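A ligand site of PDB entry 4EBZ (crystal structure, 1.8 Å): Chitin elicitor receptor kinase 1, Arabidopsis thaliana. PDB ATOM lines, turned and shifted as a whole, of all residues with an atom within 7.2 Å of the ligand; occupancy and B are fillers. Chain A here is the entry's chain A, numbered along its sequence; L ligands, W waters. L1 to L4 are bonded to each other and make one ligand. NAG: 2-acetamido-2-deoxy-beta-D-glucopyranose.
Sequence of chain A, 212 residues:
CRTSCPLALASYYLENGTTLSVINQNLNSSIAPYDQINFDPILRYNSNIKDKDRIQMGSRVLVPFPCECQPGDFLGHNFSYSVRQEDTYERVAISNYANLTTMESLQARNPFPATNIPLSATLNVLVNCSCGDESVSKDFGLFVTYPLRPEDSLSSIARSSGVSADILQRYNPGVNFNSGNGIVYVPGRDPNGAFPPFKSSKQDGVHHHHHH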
ATOM      1  N   VAL A  83     -10.128 -21.331 -16.733  1.00  0.00           N
ATOM      2  CA  VAL A  83     -10.296 -22.694 -17.211  1.00  0.00           C
ATOM      3  C   VAL A  83     -11.665 -23.276 -16.849  1.00  0.00           C
ATOM      4  O   VAL A  83     -12.181 -23.046 -15.760  1.00  0.00           O
ATOM      5  CB  VAL A  83      -9.147 -23.584 -16.640  1.00  0.00           C
ATOM      6  CG1 VAL A  83      -9.399 -25.069 -16.862  1.00  0.00           C
ATOM      7  CG2 VAL A  83      -7.788 -23.115 -17.272  1.00  0.00           C
ATOM      8  N   ARG A  84     -12.267 -24.006 -17.796  1.00  0.00           N
ATOM      9  CA  ARG A  84     -13.541 -24.677 -17.584  1.00  0.00           C
ATOM     10  C   ARG A  84     -13.368 -26.177 -17.775  1.00  0.00           C
ATOM     11  O   ARG A  84     -12.407 -26.635 -18.412  1.00  0.00           O
ATOM     12  CB  ARG A  84     -14.592 -24.158 -18.571  1.00  0.00           C
ATOM     13  CG  ARG A  84     -14.885 -22.663 -18.501  1.00  0.00           C
ATOM     14  CD  ARG A  84     -15.627 -22.190 -19.765  1.00  0.00           C
ATOM     15  NE  ARG A  84     -14.894 -22.577 -20.975  1.00  0.00           N
ATOM     16  CZ  ARG A  84     -15.186 -23.624 -21.737  1.00  0.00           C
ATOM     17  NH1 ARG A  84     -14.438 -23.911 -22.799  1.00  0.00           N
ATOM     18  NH2 ARG A  84     -16.232 -24.397 -21.449  1.00  0.00           N
ATOM     19  N   GLN A  85     -14.292 -26.961 -17.216  1.00  0.00           N
ATOM     20  CA  GLN A  85     -14.262 -28.404 -17.369  1.00  0.00           C
ATOM     21  C   GLN A  85     -13.951 -28.850 -18.806  1.00  0.00           C
ATOM     22  O   GLN A  85     -14.549 -28.353 -19.753  1.00  0.00           O
ATOM     23  CB  GLN A  85     -15.604 -28.997 -16.934  1.00  0.00           C
ATOM     24  CG  GLN A  85     -15.659 -30.502 -17.044  1.00  0.00           C
ATOM     25  CD  GLN A  85     -14.869 -31.184 -15.949  1.00  0.00           C
ATOM     26  OE1 GLN A  85     -14.351 -32.283 -16.125  1.00  0.00           O
ATOM     27  NE2 GLN A  85     -14.787 -30.526 -14.793  1.00  0.00           N
ATOM     28  N   GLU A  86     -13.007 -29.782 -18.929  1.00  0.00           N
ATOM     29  CA  GLU A  86     -12.634 -30.397 -20.204  1.00  0.00           C
ATOM     30  C   GLU A  86     -11.714 -29.547 -21.087  1.00  0.00           C
ATOM     31  O   GLU A  86     -11.326 -29.951 -22.179  1.00  0.00           O
ATOM     32  CB  GLU A  86     -13.872 -30.852 -20.973  1.00  0.00           C
ATOM     33  CG  GLU A  86     -14.855 -31.606 -20.070  1.00  0.00           C
ATOM     34  CD  GLU A  86     -15.393 -32.860 -20.700  1.00  0.00           C
ATOM     35  OE1 GLU A  86     -15.906 -32.790 -21.835  1.00  0.00           O
ATOM     36  OE2 GLU A  86     -15.304 -33.932 -20.055  1.00  0.00           O
ATOM     37  N   ASP A  87     -11.355 -28.369 -20.613  1.00  0.00           N
ATOM     38  CA  ASP A  87     -10.388 -27.568 -21.346  1.00  0.00           C
ATOM     39  C   ASP A  87      -9.031 -28.291 -21.393  1.00  0.00           C
ATOM     40  O   ASP A  87      -8.634 -28.959 -20.417  1.00  0.00           O
ATOM     41  CB  ASP A  87     -10.194 -26.200 -20.690  1.00  0.00           C
ATOM     42  CG  ASP A  87     -11.303 -25.199 -21.045  1.00  0.00           C
ATOM     43  OD1 ASP A  87     -12.100 -25.468 -21.985  1.00  0.00           O
ATOM     44  OD2 ASP A  87     -11.358 -24.138 -20.380  1.00  0.00           O
ATOM     45  N   THR A  88      -8.325 -28.174 -22.508  1.00  0.00           N
ATOM     46  CA  THR A  88      -6.938 -28.659 -22.619  1.00  0.00           C
ATOM     47  C   THR A  88      -6.120 -27.575 -23.303  1.00  0.00           C
ATOM     48  O   THR A  88      -6.677 -26.676 -23.930  1.00  0.00           O
ATOM     49  CB  THR A  88      -6.829 -29.936 -23.464  1.00  0.00           C
ATOM     50  OG1 THR A  88      -7.247 -29.668 -24.803  1.00  0.00           O
ATOM     51  CG2 THR A  88      -7.660 -31.087 -22.855  1.00  0.00           C
ATOM     52  N   TYR A  89      -4.797 -27.634 -23.206  1.00  0.00           N
ATOM     53  CA  TYR A  89      -4.007 -26.615 -23.886  1.00  0.00           C
ATOM     54  C   TYR A  89      -4.266 -26.622 -25.406  1.00  0.00           C
ATOM     55  O   TYR A  89      -4.315 -25.564 -26.041  1.00  0.00           O
ATOM     56  CB  TYR A  89      -2.512 -26.790 -23.627  1.00  0.00           C
ATOM     57  CG  TYR A  89      -2.064 -26.466 -22.204  1.00  0.00           C
ATOM     58  CD1 TYR A  89      -2.276 -25.212 -21.665  1.00  0.00           C
ATOM     59  CD2 TYR A  89      -1.365 -27.403 -21.438  1.00  0.00           C
ATOM     60  CE1 TYR A  89      -1.824 -24.880 -20.404  1.00  0.00           C
ATOM     61  CE2 TYR A  89      -0.914 -27.086 -20.160  1.00  0.00           C
ATOM     62  CZ  TYR A  89      -1.143 -25.809 -19.651  1.00  0.00           C
ATOM     63  OH  TYR A  89      -0.709 -25.464 -18.381  1.00  0.00           O
ATOM     64  N   GLU A  90      -4.430 -27.802 -25.984  1.00  0.00           N
ATOM     65  CA  GLU A  90      -4.735 -27.894 -27.410  1.00  0.00           C
ATOM     66  C   GLU A  90      -6.069 -27.209 -27.713  1.00  0.00           C
ATOM     67  O   GLU A  90      -6.165 -26.357 -28.610  1.00  0.00           O
ATOM     68  CB  GLU A  90      -4.808 -29.361 -27.870  1.00  0.00           C
ATOM     69  CG  GLU A  90      -5.141 -29.428 -29.369  1.00  0.00           C
ATOM     70  CD  GLU A  90      -5.586 -30.808 -29.836  1.00  0.00           C
ATOM     71  OE1 GLU A  90      -6.097 -31.584 -29.008  1.00  0.00           O
ATOM     72  OE2 GLU A  90      -5.421 -31.108 -31.039  1.00  0.00           O
ATOM     73  N   ARG A  91      -7.110 -27.546 -26.957  1.00  0.00           N
ATOM     74  CA  ARG A  91      -8.432 -26.962 -27.205  1.00  0.00           C
ATOM     75  C   ARG A  91      -8.445 -25.467 -26.947  1.00  0.00           C
ATOM     76  O   ARG A  91      -9.050 -24.725 -27.706  1.00  0.00           O
ATOM     77  CB  ARG A  91      -9.529 -27.639 -26.359  1.00  0.00           C
ATOM     78  CG  ARG A  91      -9.949 -28.991 -26.927  1.00  0.00           C
ATOM     79  CD  ARG A  91     -11.157 -29.594 -26.195  1.00  0.00           C
ATOM     80  NE  ARG A  91     -11.887 -28.620 -25.383  1.00  0.00           N
ATOM     81  CZ  ARG A  91     -12.944 -28.929 -24.634  1.00  0.00           C
ATOM     82  NH1 ARG A  91     -13.399 -30.179 -24.611  1.00  0.00           N
ATOM     83  NH2 ARG A  91     -13.543 -27.996 -23.900  1.00  0.00           N
ATOM     84  N   VAL A  92      -7.794 -25.025 -25.876  1.00  0.00           N
ATOM     85  CA  VAL A  92      -7.731 -23.590 -25.653  1.00  0.00           C
ATOM     86  C   VAL A  92      -7.095 -22.841 -26.829  1.00  0.00           C
ATOM     87  O   VAL A  92      -7.560 -21.759 -27.218  1.00  0.00           O
ATOM     88  CB  VAL A  92      -7.042 -23.268 -24.310  1.00  0.00           C
ATOM     89  CG1 VAL A  92      -6.834 -21.759 -24.168  1.00  0.00           C
ATOM     90  CG2 VAL A  92      -7.898 -23.826 -23.122  1.00  0.00           C
ATOM     91  N   MET A 103      -0.744 -24.165 -28.917  1.00  0.00           N
ATOM     92  CA  MET A 103      -0.669 -25.017 -27.737  1.00  0.00           C
ATOM     93  C   MET A 103       0.734 -25.007 -27.159  1.00  0.00           C
ATOM     94  O   MET A 103       0.909 -25.057 -25.933  1.00  0.00           O
ATOM     95  CB  MET A 103      -1.211 -26.433 -27.986  1.00  0.00           C
ATOM     96  CG  MET A 103      -0.562 -27.224 -29.102  1.00  0.00           C
ATOM     97  SD  MET A 103      -1.138 -28.953 -28.936  1.00  0.00           S
ATOM     98  CE  MET A 103       0.084 -29.573 -27.787  1.00  0.00           C
ATOM     99  N   GLN A 107       1.605 -24.053 -23.273  1.00  0.00           N
ATOM    100  CA  GLN A 107       2.309 -24.975 -22.389  1.00  0.00           C
ATOM    101  C   GLN A 107       3.575 -24.352 -21.805  1.00  0.00           C
ATOM    102  O   GLN A 107       3.917 -24.599 -20.650  1.00  0.00           O
ATOM    103  CB  GLN A 107       2.702 -26.247 -23.145  1.00  0.00           C
ATOM    104  CG  GLN A 107       1.566 -27.176 -23.455  1.00  0.00           C
ATOM    105  CD  GLN A 107       1.859 -28.587 -22.978  1.00  0.00           C
ATOM    106  OE1 GLN A 107       1.775 -29.535 -23.742  1.00  0.00           O
ATOM    107  NE2 GLN A 107       2.224 -28.726 -21.702  1.00  0.00           N
ATOM    108  N   PHE A 112       0.941 -25.515 -15.238  1.00  0.00           N
ATOM    109  CA  PHE A 112       0.144 -26.716 -15.000  1.00  0.00           C
ATOM    110  C   PHE A 112       0.504 -27.813 -16.013  1.00  0.00           C
ATOM    111  O   PHE A 112       0.604 -27.563 -17.210  1.00  0.00           O
ATOM    112  CB  PHE A 112      -1.374 -26.374 -15.089  1.00  0.00           C
ATOM    113  CG  PHE A 112      -1.741 -25.106 -14.371  1.00  0.00           C
ATOM    114  CD1 PHE A 112      -1.843 -25.089 -12.996  1.00  0.00           C
ATOM    115  CD2 PHE A 112      -1.985 -23.930 -15.083  1.00  0.00           C
ATOM    116  CE1 PHE A 112      -2.157 -23.910 -12.317  1.00  0.00           C
ATOM    117  CE2 PHE A 112      -2.298 -22.749 -14.421  1.00  0.00           C
ATOM    118  CZ  PHE A 112      -2.389 -22.740 -13.027  1.00  0.00           C
ATOM    119  N   PRO A 113       0.691 -29.050 -15.546  1.00  0.00           N
ATOM    120  CA  PRO A 113       0.948 -30.146 -16.496  1.00  0.00           C
ATOM    121  C   PRO A 113      -0.253 -30.295 -17.417  1.00  0.00           C
ATOM    122  O   PRO A 113      -1.386 -30.067 -16.962  1.00  0.00           O
ATOM    123  CB  PRO A 113       1.043 -31.387 -15.603  1.00  0.00           C
ATOM    124  CG  PRO A 113       1.172 -30.881 -14.205  1.00  0.00           C
ATOM    125  CD  PRO A 113       0.520 -29.531 -14.167  1.00  0.00           C
ATOM    126  N   ALA A 114      -0.054 -30.676 -18.672  1.00  0.00           N
ATOM    127  CA  ALA A 114      -1.192 -30.766 -19.594  1.00  0.00           C
ATOM    128  C   ALA A 114      -2.367 -31.599 -19.064  1.00  0.00           C
ATOM    129  O   ALA A 114      -3.525 -31.259 -19.287  1.00  0.00           O
ATOM    130  CB  ALA A 114      -0.732 -31.296 -20.952  1.00  0.00           C
ATOM    131  N   THR A 115      -2.072 -32.702 -18.377  1.00  0.00           N
ATOM    132  CA  THR A 115      -3.141 -33.597 -17.953  1.00  0.00           C
ATOM    133  C   THR A 115      -3.704 -33.270 -16.579  1.00  0.00           C
ATOM    134  O   THR A 115      -4.538 -34.013 -16.058  1.00  0.00           O
ATOM    135  CB  THR A 115      -2.693 -35.053 -17.984  1.00  0.00           C
ATOM    136  OG1 THR A 115      -1.615 -35.235 -17.056  1.00  0.00           O
ATOM    137  CG2 THR A 115      -2.258 -35.418 -19.412  1.00  0.00           C
ATOM    138  N   ASN A 116      -3.280 -32.159 -15.989  1.00  0.00           N
ATOM    139  CA  ASN A 116      -3.980 -31.643 -14.808  1.00  0.00           C
ATOM    140  C   ASN A 116      -3.965 -30.130 -14.733  1.00  0.00           C
ATOM    141  O   ASN A 116      -3.334 -29.538 -13.854  1.00  0.00           O
ATOM    142  CB  ASN A 116      -3.497 -32.240 -13.491  1.00  0.00           C
ATOM    143  CG  ASN A 116      -4.459 -31.930 -12.339  1.00  0.00           C
ATOM    144  OD1 ASN A 116      -5.597 -31.476 -12.553  1.00  0.00           O
ATOM    145  ND2 ASN A 116      -4.016 -32.155 -11.116  1.00  0.00           N
ATOM    146  N   ILE A 117      -4.678 -29.512 -15.647  1.00  0.00           N
ATOM    147  CA  ILE A 117      -5.005 -28.098 -15.522  1.00  0.00           C
ATOM    148  C   ILE A 117      -6.213 -28.026 -14.583  1.00  0.00           C
ATOM    149  O   ILE A 117      -7.286 -28.519 -14.936  1.00  0.00           O
ATOM    150  CB  ILE A 117      -5.374 -27.503 -16.859  1.00  0.00           C
ATOM    151  CG1 ILE A 117      -4.224 -27.723 -17.860  1.00  0.00           C
ATOM    152  CG2 ILE A 117      -5.647 -25.989 -16.727  1.00  0.00           C
ATOM    153  CD1 ILE A 117      -4.581 -27.328 -19.283  1.00  0.00           C
ATOM    154  N   PRO A 118      -6.055 -27.416 -13.397  1.00  0.00           N
ATOM    155  CA  PRO A 118      -7.154 -27.385 -12.406  1.00  0.00           C
ATOM    156  C   PRO A 118      -8.342 -26.491 -12.795  1.00  0.00           C
ATOM    157  O   PRO A 118      -8.190 -25.493 -13.506  1.00  0.00           O
ATOM    158  CB  PRO A 118      -6.486 -26.819 -11.139  1.00  0.00           C
ATOM    159  CG  PRO A 118      -5.084 -26.475 -11.510  1.00  0.00           C
ATOM    160  CD  PRO A 118      -4.884 -26.640 -12.975  1.00  0.00           C
ATOM    161  N   LEU A 119      -9.534 -26.841 -12.303  1.00  0.00           N
ATOM    162  CA  LEU A 119     -10.708 -26.032 -12.567  1.00  0.00           C
ATOM    163  C   LEU A 119     -10.506 -24.655 -11.938  1.00  0.00           C
ATOM    164  O   LEU A 119      -9.977 -24.552 -10.838  1.00  0.00           O
ATOM    165  CB  LEU A 119     -11.961 -26.701 -11.973  1.00  0.00           C
ATOM    166  CG  LEU A 119     -12.931 -27.436 -12.910  1.00  0.00           C
ATOM    167  CD1 LEU A 119     -12.311 -27.899 -14.214  1.00  0.00           C
ATOM    168  CD2 LEU A 119     -13.614 -28.575 -12.170  1.00  0.00           C
ATOM    169  N   SER A 120     -10.897 -23.597 -12.640  1.00  0.00           N
ATOM    170  CA  SER A 120     -10.694 -22.242 -12.141  1.00  0.00           C
ATOM    171  C   SER A 120      -9.226 -21.756 -12.069  1.00  0.00           C
ATOM    172  O   SER A 120      -8.965 -20.644 -11.617  1.00  0.00           O
ATOM    173  CB  SER A 120     -11.402 -22.038 -10.798  1.00  0.00           C
ATOM    174  OG  SER A 120     -12.811 -21.914 -10.984  1.00  0.00           O
HETATM  175  C1  NAG L   1      -4.240 -34.337 -24.994  1.00  0.00           C
HETATM  176  C2  NAG L   1      -4.134 -33.113 -24.071  1.00  0.00           C
HETATM  177  C3  NAG L   1      -4.322 -33.522 -22.609  1.00  0.00           C
HETATM  178  C4  NAG L   1      -5.586 -34.360 -22.440  1.00  0.00           C
HETATM  179  C5  NAG L   1      -5.626 -35.499 -23.466  1.00  0.00           C
HETATM  180  C6  NAG L   1      -6.951 -36.243 -23.382  1.00  0.00           C
HETATM  181  C7  NAG L   1      -2.800 -31.181 -24.664  1.00  0.00           C
HETATM  182  C8  NAG L   1      -1.439 -30.540 -24.779  1.00  0.00           C
HETATM  183  N2  NAG L   1      -2.848 -32.463 -24.282  1.00  0.00           N
HETATM  184  O1  NAG L   1      -4.164 -33.952 -26.350  1.00  0.00           O
HETATM  185  O3  NAG L   1      -4.447 -32.380 -21.767  1.00  0.00           O
HETATM  186  O4  NAG L   1      -5.603 -34.946 -21.146  1.00  0.00           O
HETATM  187  O5  NAG L   1      -5.462 -35.006 -24.793  1.00  0.00           O
HETATM  188  O6  NAG L   1      -6.811 -37.463 -24.074  1.00  0.00           O
HETATM  189  O7  NAG L   1      -3.822 -30.550 -24.918  1.00  0.00           O
HETATM  190  C1  NAG L   2      -6.732 -34.487 -20.356  1.00  0.00           C
HETATM  191  C2  NAG L   2      -6.885 -35.481 -19.196  1.00  0.00           C
HETATM  192  C3  NAG L   2      -7.920 -34.951 -18.221  1.00  0.00           C
HETATM  193  C4  NAG L   2      -7.530 -33.543 -17.788  1.00  0.00           C
HETATM  194  C5  NAG L   2      -7.264 -32.649 -19.003  1.00  0.00           C
HETATM  195  C6  NAG L   2      -6.828 -31.215 -18.633  1.00  0.00           C
HETATM  196  C7  NAG L   2      -6.381 -37.794 -19.758  1.00  0.00           C
HETATM  197  C8  NAG L   2      -6.842 -39.058 -20.413  1.00  0.00           C
HETATM  198  N2  NAG L   2      -7.265 -36.801 -19.664  1.00  0.00           N
HETATM  199  O3  NAG L   2      -7.998 -35.813 -17.096  1.00  0.00           O
HETATM  200  O4  NAG L   2      -8.590 -33.024 -17.032  1.00  0.00           O
HETATM  201  O5  NAG L   2      -6.286 -33.245 -19.838  1.00  0.00           O
HETATM  202  O6  NAG L   2      -5.717 -31.215 -17.772  1.00  0.00           O
HETATM  203  O7  NAG L   2      -5.222 -37.697 -19.352  1.00  0.00           O
HETATM  204  C1  NAG L   3      -8.344 -32.662 -15.645  1.00  0.00           C
HETATM  205  C2  NAG L   3      -9.378 -31.662 -15.127  1.00  0.00           C
HETATM  206  C3  NAG L   3      -9.259 -31.510 -13.616  1.00  0.00           C
HETATM  207  C4  NAG L   3      -9.285 -32.884 -12.969  1.00  0.00           C
HETATM  208  C5  NAG L   3      -8.308 -33.859 -13.592  1.00  0.00           C
HETATM  209  C6  NAG L   3      -8.584 -35.239 -12.988  1.00  0.00           C
HETATM  210  C7  NAG L   3     -10.064 -29.967 -16.700  1.00  0.00           C
HETATM  211  C8  NAG L   3      -9.796 -28.585 -17.211  1.00  0.00           C
HETATM  212  N2  NAG L   3      -9.183 -30.395 -15.788  1.00  0.00           N
HETATM  213  O3  NAG L   3     -10.350 -30.766 -13.109  1.00  0.00           O
HETATM  214  O4  NAG L   3      -8.978 -32.797 -11.583  1.00  0.00           O
HETATM  215  O5  NAG L   3      -8.444 -33.918 -14.994  1.00  0.00           O
HETATM  216  O6  NAG L   3      -7.436 -36.000 -13.262  1.00  0.00           O
HETATM  217  O7  NAG L   3     -11.018 -30.652 -17.107  1.00  0.00           O
HETATM  218  C1  NAG L   4     -10.042 -33.255 -10.691  1.00  0.00           C
HETATM  219  C2  NAG L   4      -9.354 -33.380  -9.338  1.00  0.00           C
HETATM  220  C3  NAG L   4     -10.338 -33.755  -8.221  1.00  0.00           C
HETATM  221  C4  NAG L   4     -11.593 -32.895  -8.288  1.00  0.00           C
HETATM  222  C5  NAG L   4     -12.167 -32.898  -9.697  1.00  0.00           C
HETATM  223  C6  NAG L   4     -13.395 -31.999  -9.817  1.00  0.00           C
HETATM  224  C7  NAG L   4      -7.031 -34.164  -9.211  1.00  0.00           C
HETATM  225  C8  NAG L   4      -6.136 -35.362  -9.157  1.00  0.00           C
HETATM  226  N2  NAG L   4      -8.318 -34.403  -9.426  1.00  0.00           N
HETATM  227  O3  NAG L   4      -9.710 -33.579  -6.987  1.00  0.00           O
HETATM  228  O4  NAG L   4     -12.554 -33.415  -7.380  1.00  0.00           O
HETATM  229  O5  NAG L   4     -11.198 -32.441 -10.619  1.00  0.00           O
HETATM  230  O6  NAG L   4     -14.027 -32.240 -11.043  1.00  0.00           O
HETATM  231  O7  NAG L   4      -6.573 -33.024  -9.047  1.00  0.00           O
HETATM  232  O   HOH W   1      -7.097 -30.401 -10.505  1.00  0.00           O
HETATM  233  O   HOH W   2     -12.008 -33.198 -17.973  1.00  0.00           O
HETATM  234  O   HOH W   3      -0.540 -33.950 -23.602  1.00  0.00           O
HETATM  235  O   HOH W   4     -12.725 -31.985 -13.438  1.00  0.00           O
HETATM  236  O   HOH W   5     -16.402 -30.071 -10.312  1.00  0.00           O
HETATM  237  O   HOH W   6      -3.730 -29.810 -21.675  1.00  0.00           O
HETATM  238  O   HOH W   7      -2.086 -32.383 -28.302  1.00  0.00           O
HETATM  239  O   HOH W   8      -9.601 -29.495 -10.917  1.00  0.00           O
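Val 83 touches the ligand.
O of Arg 84 touches C8 of NAG L3, 3.5 Å away.
OE1 of Gln 85 touches O7 of NAG L3, 3.8 Å away.
Asp 87 touches the ligand.
CB of Thr 88 touches O7 of NAG L1, 3.4 Å away.
Tyr 89 touches the ligand.
Met 103 touches the ligand.
OE1 of Gln 107 touches C8 of NAG L1, at 3.5 Å.
CD1 of Leu 119 touches O3 of NAG L3, at 3.6 Å.
O of Ala 114 is in hydrogen-bond range of O6 of NAG L2 (2.7 Å).
An oxygen (O6) of NAG L2 lies close to the backbone carbonyl oxygen of Thr 115.
O of Ile 117 lies within hydrogen-bond range of N2 of NAG L3 (2.8 Å).
An oxygen (O7) of NAG L1 lies within hydrogen-bond range of the backbone NH (N) of Glu 90, 3.0 Å away.
The backbone NH of Asn 116 sits at hydrogen-bond distance from an oxygen (O6) of NAG L2 (3.2 Å).
The side-chain amide nitrogen (ND2) of Asn 116 sits at hydrogen-bond distance from an oxygen (O7) of NAG L4, 3.4 Å away.
O7 of NAG L3 lies within hydrogen-bond range of N of Glu 86 (2.8 Å).
N of Ile 117 lies within hydrogen-bond range of O6 of NAG L2 (2.9 Å).
Water W8 bridges O3 of NAG L3 (2.6 Å) and N of Leu 119 (3.0 Å).
Water W6 lies within hydrogen-bond range of O3 of NAG L1 (2.7 Å), O of Ala 114 (2.8 Å) and N of Tyr 89 (2.9 Å).
Water W4 bridges an oxygen (O3) of NAG L3 (2.7 Å) and the side-chain amide nitrogen of Gln 85 (2.9 Å).
Water W2 lies within hydrogen-bond range of an oxygen (O7) of NAG L3 (2.9 Å) and the side-chain amide oxygen (OE1) of Gln 85 (3.1 Å).
Water W1 bridges OD1 of Asn 116 (2.8 Å) and O7 of NAG L4 (3.0 Å).
Water W7 lies within hydrogen-bond range of an oxygen (O1) of NAG L1 (3.3 Å) and the side-chain sulfur of Met 103 (3.6 Å).
The side-chain hydroxyl (OH) of Tyr 89 is in hydrogen-bond range of the backbone carbonyl oxygen (O) of Phe 112.
The guanidinium group of Arg 84 is in salt-bridge range of the side-chain carboxylate of Asp 87.
The guanidinium group (NH2) of Arg 91 is in salt-bridge range of the side-chain carboxylate (OD1) of Asp 87.
The backbone carbonyl oxygen (O) of Glu 86 lies close to the guanidinium group (NH1) of Arg 91 (3.2 Å).
The side-chain hydroxyl of Thr 88 is in hydrogen-bond range of the backbone NH of Arg 91.
O of Val 83 lies within hydrogen-bond range of N of Ser 120 (3.4 Å).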
